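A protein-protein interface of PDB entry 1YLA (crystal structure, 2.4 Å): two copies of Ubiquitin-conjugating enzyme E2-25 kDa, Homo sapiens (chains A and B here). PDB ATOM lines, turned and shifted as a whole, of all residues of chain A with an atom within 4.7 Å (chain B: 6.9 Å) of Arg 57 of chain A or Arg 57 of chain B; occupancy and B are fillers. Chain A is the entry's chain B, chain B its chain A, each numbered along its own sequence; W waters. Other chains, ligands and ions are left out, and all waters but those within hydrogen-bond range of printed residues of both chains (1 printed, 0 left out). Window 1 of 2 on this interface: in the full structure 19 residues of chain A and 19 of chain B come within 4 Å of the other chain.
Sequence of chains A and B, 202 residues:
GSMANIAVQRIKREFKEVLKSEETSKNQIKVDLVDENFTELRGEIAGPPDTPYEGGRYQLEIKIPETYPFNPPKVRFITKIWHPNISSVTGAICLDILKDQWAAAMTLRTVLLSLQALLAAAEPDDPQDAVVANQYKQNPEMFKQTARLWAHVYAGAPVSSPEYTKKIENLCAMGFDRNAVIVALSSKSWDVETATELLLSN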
ATOM      1  N   GLU A  44      17.325 -25.731 -29.315  1.00  0.00           N
ATOM      2  CA  GLU A  44      18.427 -25.238 -30.116  1.00  0.00           C
ATOM      3  C   GLU A  44      18.395 -26.006 -31.425  1.00  0.00           C
ATOM      4  O   GLU A  44      18.507 -27.231 -31.433  1.00  0.00           O
ATOM      5  CB  GLU A  44      19.775 -25.453 -29.421  1.00  0.00           C
ATOM      6  CG  GLU A  44      20.935 -24.837 -30.208  1.00  0.00           C
ATOM      7  CD  GLU A  44      22.260 -24.869 -29.470  1.00  0.00           C
ATOM      8  OE1 GLU A  44      22.304 -24.421 -28.310  1.00  0.00           O
ATOM      9  OE2 GLU A  44      23.267 -25.335 -30.052  1.00  0.00           O
ATOM     10  N   ILE A  45      18.209 -25.293 -32.528  1.00  0.00           N
ATOM     11  CA  ILE A  45      18.165 -25.923 -33.841  1.00  0.00           C
ATOM     12  C   ILE A  45      19.379 -25.492 -34.664  1.00  0.00           C
ATOM     13  O   ILE A  45      19.929 -24.414 -34.460  1.00  0.00           O
ATOM     14  CB  ILE A  45      16.843 -25.574 -34.589  1.00  0.00           C
ATOM     15  CG1 ILE A  45      16.686 -24.053 -34.704  1.00  0.00           C
ATOM     16  CG2 ILE A  45      15.648 -26.190 -33.850  1.00  0.00           C
ATOM     17  CD1 ILE A  45      15.404 -23.607 -35.383  1.00  0.00           C
ATOM     18  N   GLY A  55      25.726 -22.897 -40.315  1.00  0.00           N
ATOM     19  CA  GLY A  55      26.856 -22.683 -39.431  1.00  0.00           C
ATOM     20  C   GLY A  55      26.429 -22.049 -38.124  1.00  0.00           C
ATOM     21  O   GLY A  55      27.206 -21.969 -37.175  1.00  0.00           O
ATOM     22  N   GLY A  56      25.186 -21.592 -38.079  1.00  0.00           N
ATOM     23  CA  GLY A  56      24.679 -20.971 -36.875  1.00  0.00           C
ATOM     24  C   GLY A  56      23.828 -21.929 -36.069  1.00  0.00           C
ATOM     25  O   GLY A  56      23.226 -22.861 -36.624  1.00  0.00           O
ATOM     26  N   ARG A  57      23.803 -21.709 -34.754  1.00  0.00           N
ATOM     27  CA  ARG A  57      23.011 -22.519 -33.826  1.00  0.00           C
ATOM     28  C   ARG A  57      22.019 -21.562 -33.211  1.00  0.00           C
ATOM     29  O   ARG A  57      22.397 -20.493 -32.733  1.00  0.00           O
ATOM     30  CB  ARG A  57      23.892 -23.124 -32.734  1.00  0.00           C
ATOM     31  CG  ARG A  57      25.049 -23.917 -33.270  1.00  0.00           C
ATOM     32  CD  ARG A  57      25.729 -24.707 -32.184  1.00  0.00           C
ATOM     33  NE  ARG A  57      26.926 -25.355 -32.701  1.00  0.00           N
ATOM     34  CZ  ARG A  57      27.920 -25.793 -31.942  1.00  0.00           C
ATOM     35  NH1 ARG A  57      27.848 -25.650 -30.627  1.00  0.00           N
ATOM     36  NH2 ARG A  57      28.987 -26.356 -32.498  1.00  0.00           N
ATOM     37  N   TYR A  58      20.755 -21.952 -33.204  1.00  0.00           N
ATOM     38  CA  TYR A  58      19.711 -21.081 -32.699  1.00  0.00           C
ATOM     39  C   TYR A  58      18.973 -21.570 -31.460  1.00  0.00           C
ATOM     40  O   TYR A  58      18.351 -22.624 -31.479  1.00  0.00           O
ATOM     41  CB  TYR A  58      18.706 -20.803 -33.867  1.00  0.00           C
ATOM     42  CG  TYR A  58      19.395 -20.062 -34.971  1.00  0.00           C
ATOM     43  CD1 TYR A  58      19.509 -18.663 -34.941  1.00  0.00           C
ATOM     44  CD2 TYR A  58      19.953 -20.736 -36.070  1.00  0.00           C
ATOM     45  CE1 TYR A  58      20.190 -17.970 -35.936  1.00  0.00           C
ATOM     46  CE2 TYR A  58      20.643 -20.039 -37.080  1.00  0.00           C
ATOM     47  CZ  TYR A  58      20.755 -18.661 -36.995  1.00  0.00           C
ATOM     48  OH  TYR A  58      21.441 -17.966 -37.965  1.00  0.00           O
ATOM     49  N   GLN A  59      19.037 -20.789 -30.385  1.00  0.00           N
ATOM     50  CA  GLN A  59      18.356 -21.147 -29.149  1.00  0.00           C
ATOM     51  C   GLN A  59      16.918 -20.678 -29.155  1.00  0.00           C
ATOM     52  O   GLN A  59      16.598 -19.620 -29.684  1.00  0.00           O
ATOM     53  CB  GLN A  59      19.091 -20.566 -27.947  1.00  0.00           C
ATOM     54  CG  GLN A  59      20.367 -21.314 -27.651  1.00  0.00           C
ATOM     55  CD  GLN A  59      21.196 -20.645 -26.601  1.00  0.00           C
ATOM     56  OE1 GLN A  59      20.696 -20.282 -25.538  1.00  0.00           O
ATOM     57  NE2 GLN A  59      22.483 -20.481 -26.883  1.00  0.00           N
ATOM     58  N   THR A  79      18.103 -16.441 -29.915  1.00  0.00           N
ATOM     59  CA  THR A  79      19.211 -16.034 -30.758  1.00  0.00           C
ATOM     60  C   THR A  79      18.619 -15.188 -31.877  1.00  0.00           C
ATOM     61  O   THR A  79      17.731 -15.653 -32.604  1.00  0.00           O
ATOM     62  CB  THR A  79      19.912 -17.262 -31.364  1.00  0.00           C
ATOM     63  OG1 THR A  79      20.406 -18.086 -30.303  1.00  0.00           O
ATOM     64  CG2 THR A  79      21.075 -16.837 -32.271  1.00  0.00           C
ATOM     65  N   ALA A 155      24.621 -16.195 -34.279  1.00  0.00           N
ATOM     66  CA  ALA A 155      24.514 -17.661 -34.308  1.00  0.00           C
ATOM     67  C   ALA A 155      25.839 -18.416 -34.453  1.00  0.00           C
ATOM     68  O   ALA A 155      25.890 -19.649 -34.284  1.00  0.00           O
ATOM     69  CB  ALA A 155      23.550 -18.086 -35.417  1.00  0.00           C
ATOM     70  N   GLY A 156      26.903 -17.688 -34.783  1.00  0.00           N
ATOM     71  CA  GLY A 156      28.206 -18.310 -34.916  1.00  0.00           C
ATOM     72  C   GLY A 156      28.547 -18.929 -36.258  1.00  0.00           C
ATOM     73  O   GLY A 156      29.384 -19.833 -36.321  1.00  0.00           O
ATOM     74  N   ASN B  27      35.447 -16.723 -35.418  1.00  0.00           N
ATOM     75  CA  ASN B  27      34.575 -17.371 -34.441  1.00  0.00           C
ATOM     76  C   ASN B  27      35.273 -18.119 -33.306  1.00  0.00           C
ATOM     77  O   ASN B  27      34.846 -19.205 -32.944  1.00  0.00           O
ATOM     78  CB  ASN B  27      33.617 -18.333 -35.137  1.00  0.00           C
ATOM     79  CG  ASN B  27      32.736 -17.640 -36.140  1.00  0.00           C
ATOM     80  OD1 ASN B  27      33.119 -17.459 -37.290  1.00  0.00           O
ATOM     81  ND2 ASN B  27      31.554 -17.226 -35.706  1.00  0.00           N
ATOM     82  N   GLU B  44      31.512 -16.309 -25.008  1.00  0.00           N
ATOM     83  CA  GLU B  44      31.397 -17.593 -25.651  1.00  0.00           C
ATOM     84  C   GLU B  44      32.722 -17.913 -26.322  1.00  0.00           C
ATOM     85  O   GLU B  44      33.223 -17.122 -27.124  1.00  0.00           O
ATOM     86  CB  GLU B  44      30.283 -17.590 -26.689  1.00  0.00           C
ATOM     87  CG  GLU B  44      30.049 -18.983 -27.232  1.00  0.00           C
ATOM     88  CD  GLU B  44      28.957 -19.043 -28.241  1.00  0.00           C
ATOM     89  OE1 GLU B  44      27.810 -18.690 -27.893  1.00  0.00           O
ATOM     90  OE2 GLU B  44      29.248 -19.442 -29.390  1.00  0.00           O
ATOM     91  N   ILE B  45      33.307 -19.053 -25.970  1.00  0.00           N
ATOM     92  CA  ILE B  45      34.565 -19.464 -26.569  1.00  0.00           C
ATOM     93  C   ILE B  45      34.322 -20.784 -27.284  1.00  0.00           C
ATOM     94  O   ILE B  45      33.428 -21.550 -26.920  1.00  0.00           O
ATOM     95  CB  ILE B  45      35.716 -19.638 -25.508  1.00  0.00           C
ATOM     96  CG1 ILE B  45      35.289 -20.623 -24.413  1.00  0.00           C
ATOM     97  CG2 ILE B  45      36.108 -18.272 -24.910  1.00  0.00           C
ATOM     98  CD1 ILE B  45      36.315 -20.804 -23.306  1.00  0.00           C
ATOM     99  N   ALA B  46      35.115 -21.027 -28.318  1.00  0.00           N
ATOM    100  CA  ALA B  46      35.007 -22.236 -29.109  1.00  0.00           C
ATOM    101  C   ALA B  46      35.938 -23.269 -28.509  1.00  0.00           C
ATOM    102  O   ALA B  46      37.031 -22.926 -28.056  1.00  0.00           O
ATOM    103  CB  ALA B  46      35.410 -21.943 -30.545  1.00  0.00           C
ATOM    104  N   GLY B  47      35.519 -24.530 -28.494  1.00  0.00           N
ATOM    105  CA  GLY B  47      36.390 -25.555 -27.948  1.00  0.00           C
ATOM    106  C   GLY B  47      37.650 -25.657 -28.798  1.00  0.00           C
ATOM    107  O   GLY B  47      37.556 -25.674 -30.026  1.00  0.00           O
ATOM    108  N   TYR B  53      36.913 -30.959 -26.379  1.00  0.00           N
ATOM    109  CA  TYR B  53      36.040 -29.799 -26.486  1.00  0.00           C
ATOM    110  C   TYR B  53      35.914 -29.284 -27.916  1.00  0.00           C
ATOM    111  O   TYR B  53      35.157 -28.355 -28.177  1.00  0.00           O
ATOM    112  CB  TYR B  53      36.559 -28.695 -25.565  1.00  0.00           C
ATOM    113  CG  TYR B  53      36.913 -29.213 -24.189  1.00  0.00           C
ATOM    114  CD1 TYR B  53      38.240 -29.256 -23.762  1.00  0.00           C
ATOM    115  CD2 TYR B  53      35.926 -29.723 -23.336  1.00  0.00           C
ATOM    116  CE1 TYR B  53      38.587 -29.794 -22.536  1.00  0.00           C
ATOM    117  CE2 TYR B  53      36.263 -30.264 -22.103  1.00  0.00           C
ATOM    118  CZ  TYR B  53      37.598 -30.297 -21.714  1.00  0.00           C
ATOM    119  OH  TYR B  53      37.953 -30.837 -20.507  1.00  0.00           O
ATOM    120  N   GLU B  54      36.649 -29.891 -28.841  1.00  0.00           N
ATOM    121  CA  GLU B  54      36.590 -29.492 -30.242  1.00  0.00           C
ATOM    122  C   GLU B  54      35.180 -29.696 -30.813  1.00  0.00           C
ATOM    123  O   GLU B  54      34.615 -30.787 -30.739  1.00  0.00           O
ATOM    124  CB  GLU B  54      37.579 -30.307 -31.065  1.00  0.00           C
ATOM    125  CG  GLU B  54      37.930 -29.644 -32.377  1.00  0.00           C
ATOM    126  CD  GLU B  54      38.582 -30.592 -33.362  1.00  0.00           C
ATOM    127  OE1 GLU B  54      39.561 -31.271 -32.991  1.00  0.00           O
ATOM    128  OE2 GLU B  54      38.116 -30.653 -34.519  1.00  0.00           O
ATOM    129  N   GLY B  55      34.619 -28.644 -31.393  1.00  0.00           N
ATOM    130  CA  GLY B  55      33.285 -28.739 -31.951  1.00  0.00           C
ATOM    131  C   GLY B  55      32.306 -28.054 -31.025  1.00  0.00           C
ATOM    132  O   GLY B  55      31.195 -27.681 -31.424  1.00  0.00           O
ATOM    133  N   GLY B  56      32.738 -27.888 -29.778  1.00  0.00           N
ATOM    134  CA  GLY B  56      31.911 -27.240 -28.780  1.00  0.00           C
ATOM    135  C   GLY B  56      32.076 -25.727 -28.707  1.00  0.00           C
ATOM    136  O   GLY B  56      33.113 -25.155 -29.088  1.00  0.00           O
ATOM    137  N   ARG B  57      31.010 -25.095 -28.221  1.00  0.00           N
ATOM    138  CA  ARG B  57      30.917 -23.656 -28.029  1.00  0.00           C
ATOM    139  C   ARG B  57      30.482 -23.507 -26.576  1.00  0.00           C
ATOM    140  O   ARG B  57      29.478 -24.104 -26.158  1.00  0.00           O
ATOM    141  CB  ARG B  57      29.860 -23.057 -28.962  1.00  0.00           C
ATOM    142  CG  ARG B  57      30.195 -23.170 -30.438  1.00  0.00           C
ATOM    143  CD  ARG B  57      29.147 -22.504 -31.300  1.00  0.00           C
ATOM    144  NE  ARG B  57      29.306 -22.862 -32.706  1.00  0.00           N
ATOM    145  CZ  ARG B  57      28.511 -22.433 -33.679  1.00  0.00           C
ATOM    146  NH1 ARG B  57      27.498 -21.618 -33.406  1.00  0.00           N
ATOM    147  NH2 ARG B  57      28.717 -22.841 -34.923  1.00  0.00           N
ATOM    148  N   TYR B  58      31.232 -22.709 -25.816  1.00  0.00           N
ATOM    149  CA  TYR B  58      30.972 -22.528 -24.392  1.00  0.00           C
ATOM    150  C   TYR B  58      30.603 -21.120 -23.964  1.00  0.00           C
ATOM    151  O   TYR B  58      31.416 -20.199 -24.077  1.00  0.00           O
ATOM    152  CB  TYR B  58      32.216 -23.010 -23.607  1.00  0.00           C
ATOM    153  CG  TYR B  58      32.443 -24.477 -23.860  1.00  0.00           C
ATOM    154  CD1 TYR B  58      31.712 -25.446 -23.163  1.00  0.00           C
ATOM    155  CD2 TYR B  58      33.358 -24.917 -24.828  1.00  0.00           C
ATOM    156  CE1 TYR B  58      31.851 -26.799 -23.449  1.00  0.00           C
ATOM    157  CE2 TYR B  58      33.502 -26.279 -25.122  1.00  0.00           C
ATOM    158  CZ  TYR B  58      32.741 -27.209 -24.426  1.00  0.00           C
ATOM    159  OH  TYR B  58      32.876 -28.562 -24.678  1.00  0.00           O
ATOM    160  N   GLN B  59      29.383 -20.954 -23.460  1.00  0.00           N
ATOM    161  CA  GLN B  59      28.929 -19.644 -22.998  1.00  0.00           C
ATOM    162  C   GLN B  59      29.442 -19.339 -21.601  1.00  0.00           C
ATOM    163  O   GLN B  59      29.478 -20.204 -20.730  1.00  0.00           O
ATOM    164  CB  GLN B  59      27.406 -19.554 -23.030  1.00  0.00           C
ATOM    165  CG  GLN B  59      26.869 -19.681 -24.437  1.00  0.00           C
ATOM    166  CD  GLN B  59      25.384 -19.467 -24.525  1.00  0.00           C
ATOM    167  OE1 GLN B  59      24.758 -19.847 -25.515  1.00  0.00           O
ATOM    168  NE2 GLN B  59      24.804 -18.848 -23.499  1.00  0.00           N
ATOM    169  N   THR B  79      27.711 -23.041 -19.963  1.00  0.00           N
ATOM    170  CA  THR B  79      27.616 -24.315 -20.654  1.00  0.00           C
ATOM    171  C   THR B  79      28.378 -25.331 -19.807  1.00  0.00           C
ATOM    172  O   THR B  79      29.549 -25.094 -19.454  1.00  0.00           O
ATOM    173  CB  THR B  79      28.268 -24.208 -22.056  1.00  0.00           C
ATOM    174  OG1 THR B  79      27.676 -23.113 -22.765  1.00  0.00           O
ATOM    175  CG2 THR B  79      28.065 -25.486 -22.857  1.00  0.00           C
ATOM    176  N   ALA B 151      30.884 -32.468 -24.035  1.00  0.00           N
ATOM    177  CA  ALA B 151      30.995 -31.472 -25.103  1.00  0.00           C
ATOM    178  C   ALA B 151      29.855 -31.657 -26.115  1.00  0.00           C
ATOM    179  O   ALA B 151      29.259 -30.678 -26.573  1.00  0.00           O
ATOM    180  CB  ALA B 151      32.377 -31.576 -25.803  1.00  0.00           C
ATOM    181  N   TYR B 154      26.178 -30.968 -24.137  1.00  0.00           N
ATOM    182  CA  TYR B 154      26.015 -29.600 -23.643  1.00  0.00           C
ATOM    183  C   TYR B 154      26.575 -28.475 -24.520  1.00  0.00           C
ATOM    184  O   TYR B 154      26.095 -27.346 -24.447  1.00  0.00           O
ATOM    185  CB  TYR B 154      26.636 -29.472 -22.246  1.00  0.00           C
ATOM    186  CG  TYR B 154      26.014 -30.358 -21.184  1.00  0.00           C
ATOM    187  CD1 TYR B 154      26.761 -31.349 -20.550  1.00  0.00           C
ATOM    188  CD2 TYR B 154      24.680 -30.199 -20.810  1.00  0.00           C
ATOM    189  CE1 TYR B 154      26.195 -32.155 -19.572  1.00  0.00           C
ATOM    190  CE2 TYR B 154      24.101 -30.996 -19.833  1.00  0.00           C
ATOM    191  CZ  TYR B 154      24.861 -31.971 -19.216  1.00  0.00           C
ATOM    192  OH  TYR B 154      24.290 -32.752 -18.235  1.00  0.00           O
ATOM    193  N   ALA B 155      27.575 -28.770 -25.348  1.00  0.00           N
ATOM    194  CA  ALA B 155      28.197 -27.734 -26.176  1.00  0.00           C
ATOM    195  C   ALA B 155      28.146 -27.935 -27.696  1.00  0.00           C
ATOM    196  O   ALA B 155      28.866 -27.261 -28.444  1.00  0.00           O
ATOM    197  CB  ALA B 155      29.645 -27.542 -25.736  1.00  0.00           C
ATOM    198  N   GLY B 156      27.311 -28.870 -28.148  1.00  0.00           N
ATOM    199  CA  GLY B 156      27.166 -29.127 -29.569  1.00  0.00           C
ATOM    200  C   GLY B 156      28.297 -29.829 -30.305  1.00  0.00           C
ATOM    201  O   GLY B 156      28.257 -29.897 -31.532  1.00  0.00           O
ATOM    202  N   ALA B 157      29.300 -30.345 -29.597  1.00  0.00           N
ATOM    203  CA  ALA B 157      30.406 -31.040 -30.263  1.00  0.00           C
ATOM    204  C   ALA B 157      29.857 -32.243 -31.039  1.00  0.00           C
ATOM    205  O   ALA B 157      28.769 -32.740 -30.740  1.00  0.00           O
ATOM    206  CB  ALA B 157      31.445 -31.489 -29.239  1.00  0.00           C
ATOM    207  N   PRO B 158      30.601 -32.720 -32.055  1.00  0.00           N
ATOM    208  CA  PRO B 158      30.194 -33.861 -32.885  1.00  0.00           C
ATOM    209  C   PRO B 158      29.336 -34.936 -32.213  1.00  0.00           C
ATOM    210  O   PRO B 158      28.121 -34.962 -32.415  1.00  0.00           O
ATOM    211  CB  PRO B 158      31.524 -34.385 -33.399  1.00  0.00           C
ATOM    212  CG  PRO B 158      32.239 -33.099 -33.692  1.00  0.00           C
ATOM    213  CD  PRO B 158      31.939 -32.248 -32.458  1.00  0.00           C
HETATM  214  O   HOH W   1      24.394 -25.521 -26.566  1.00  0.00           O
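Gly 55 of chain A touches Arg 57 of chain B, and with the chains exchanged Arg 57 of chain A touches Gly 55 of chain B. Arg 57 of chain A touches Ala 155 of chain B, and with the chains exchanged Ala 155 of chain A touches Arg 57 of chain B. Arg 57 of chain A touches Gly 156 of chain B, and with the chains exchanged Gly 156 of chain A touches Arg 57 of chain B. Gln 59 of chain A touches its own counterpart, Gln 59 of chain B. 10 positions are printed for both chains. Of the 9 pairs that touch across the chains among the printed residues, 8 have their exchanged pair printed and touching as well.
Arg 57 of chain B touches just these residues of chain A: Gly 55 (2.8 Å), Arg 57 (3.3 Å), Ala 155 (2.7 Å) and Gly 156 (3.4 Å). Of the printed residues of chain A, Asn 27 of chain B touches Gly 156. Printed residues of chain B within 4 Å of Gly 156 of chain A: Asn 27 (3.4 Å) and Arg 57 (3.4 Å). Of the printed residues of chain A, Ala 155 of chain B touches Arg 57. Of the printed residues of chain B, Ala 155 of chain A touches Arg 57. Tyr 58 of chain A touches none of the printed residues of chain B. The nearest residue of chain B that does not touch Arg 57 of chain A is Gly 56 of chain B (4.6 Å). The nearest residue of chain A that does not touch Arg 57 of chain B is Gly 56 of chain A (4.5 Å).
Water W1 lies within hydrogen-bond range of OE1 of Glu 44 of chain A and O of Tyr 154 of chain B.
Gly 156 of chain B touches Arg 57 of chain A (CA to NH1, 3.7 Å).
The backbone carbonyl oxygen (O) of Gly 156 of chain A lies within hydrogen-bond range of the side-chain amide nitrogen (ND2) of Asn 27 of chain B (3.4 Å). The backbone carbonyl oxygen (O) of Gly 55 of chain B sits at hydrogen-bond distance from the guanidinium group (NH2) of Arg 57 of chain A, 2.8 Å away. The guanidinium group (NH2) of Arg 57 of chain B sits at hydrogen-bond distance from the backbone carbonyl oxygen (O) of Gly 55 of chain A (2.8 Å). NH1 of Arg 57 of chain B lies within hydrogen-bond range of O of Ala 155 of chain A (2.7 Å). The guanidinium group (NH2) of Arg 57 of chain B sits at hydrogen-bond distance from the backbone carbonyl oxygen (O) of Gly 156 of chain A, 3.4 Å away. The side-chain amide nitrogen (NE2) of Gln 59 of chain A sits at hydrogen-bond distance from the side-chain amide oxygen (OE1) of Gln 59 of chain B (2.7 Å). O of Ala 155 of chain B lies within hydrogen-bond range of NH1 of Arg 57 of chain A, 2.9 Å away. The guanidinium group (NE) of Arg 57 of chain A lies close to the guanidinium group (NE) of Arg 57 of chain B (3.4 Å).
Of the 10 printed residues of chain A, 5 touch a printed residue of chain B. Printed residues of chain A that touch a printed residue of chain B: Gly 55, Arg 57, Gln 59, Ala 155 and Gly 156. Of the 19 printed residues of chain B, 6 touch a printed residue of chain A.
N of Arg 57 of chain B sits at hydrogen-bond distance from O of Ala 155 of chain B (3.1 Å). OG1 of Thr 79 of chain B lies within hydrogen-bond range of N of Gln 59 of chain B, at 2.8 Å. The backbone carbonyl oxygen (O) of Ala 151 of chain B is in hydrogen-bond range of the backbone NH (N) of Gly 156 of chain B (3.1 Å). O of Ala 155 of chain A is in hydrogen-bond range of N of Arg 57 of chain A. N of Gln 59 of chain A is in hydrogen-bond range of OG1 of Thr 79 of chain A, 3.0 Å away.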
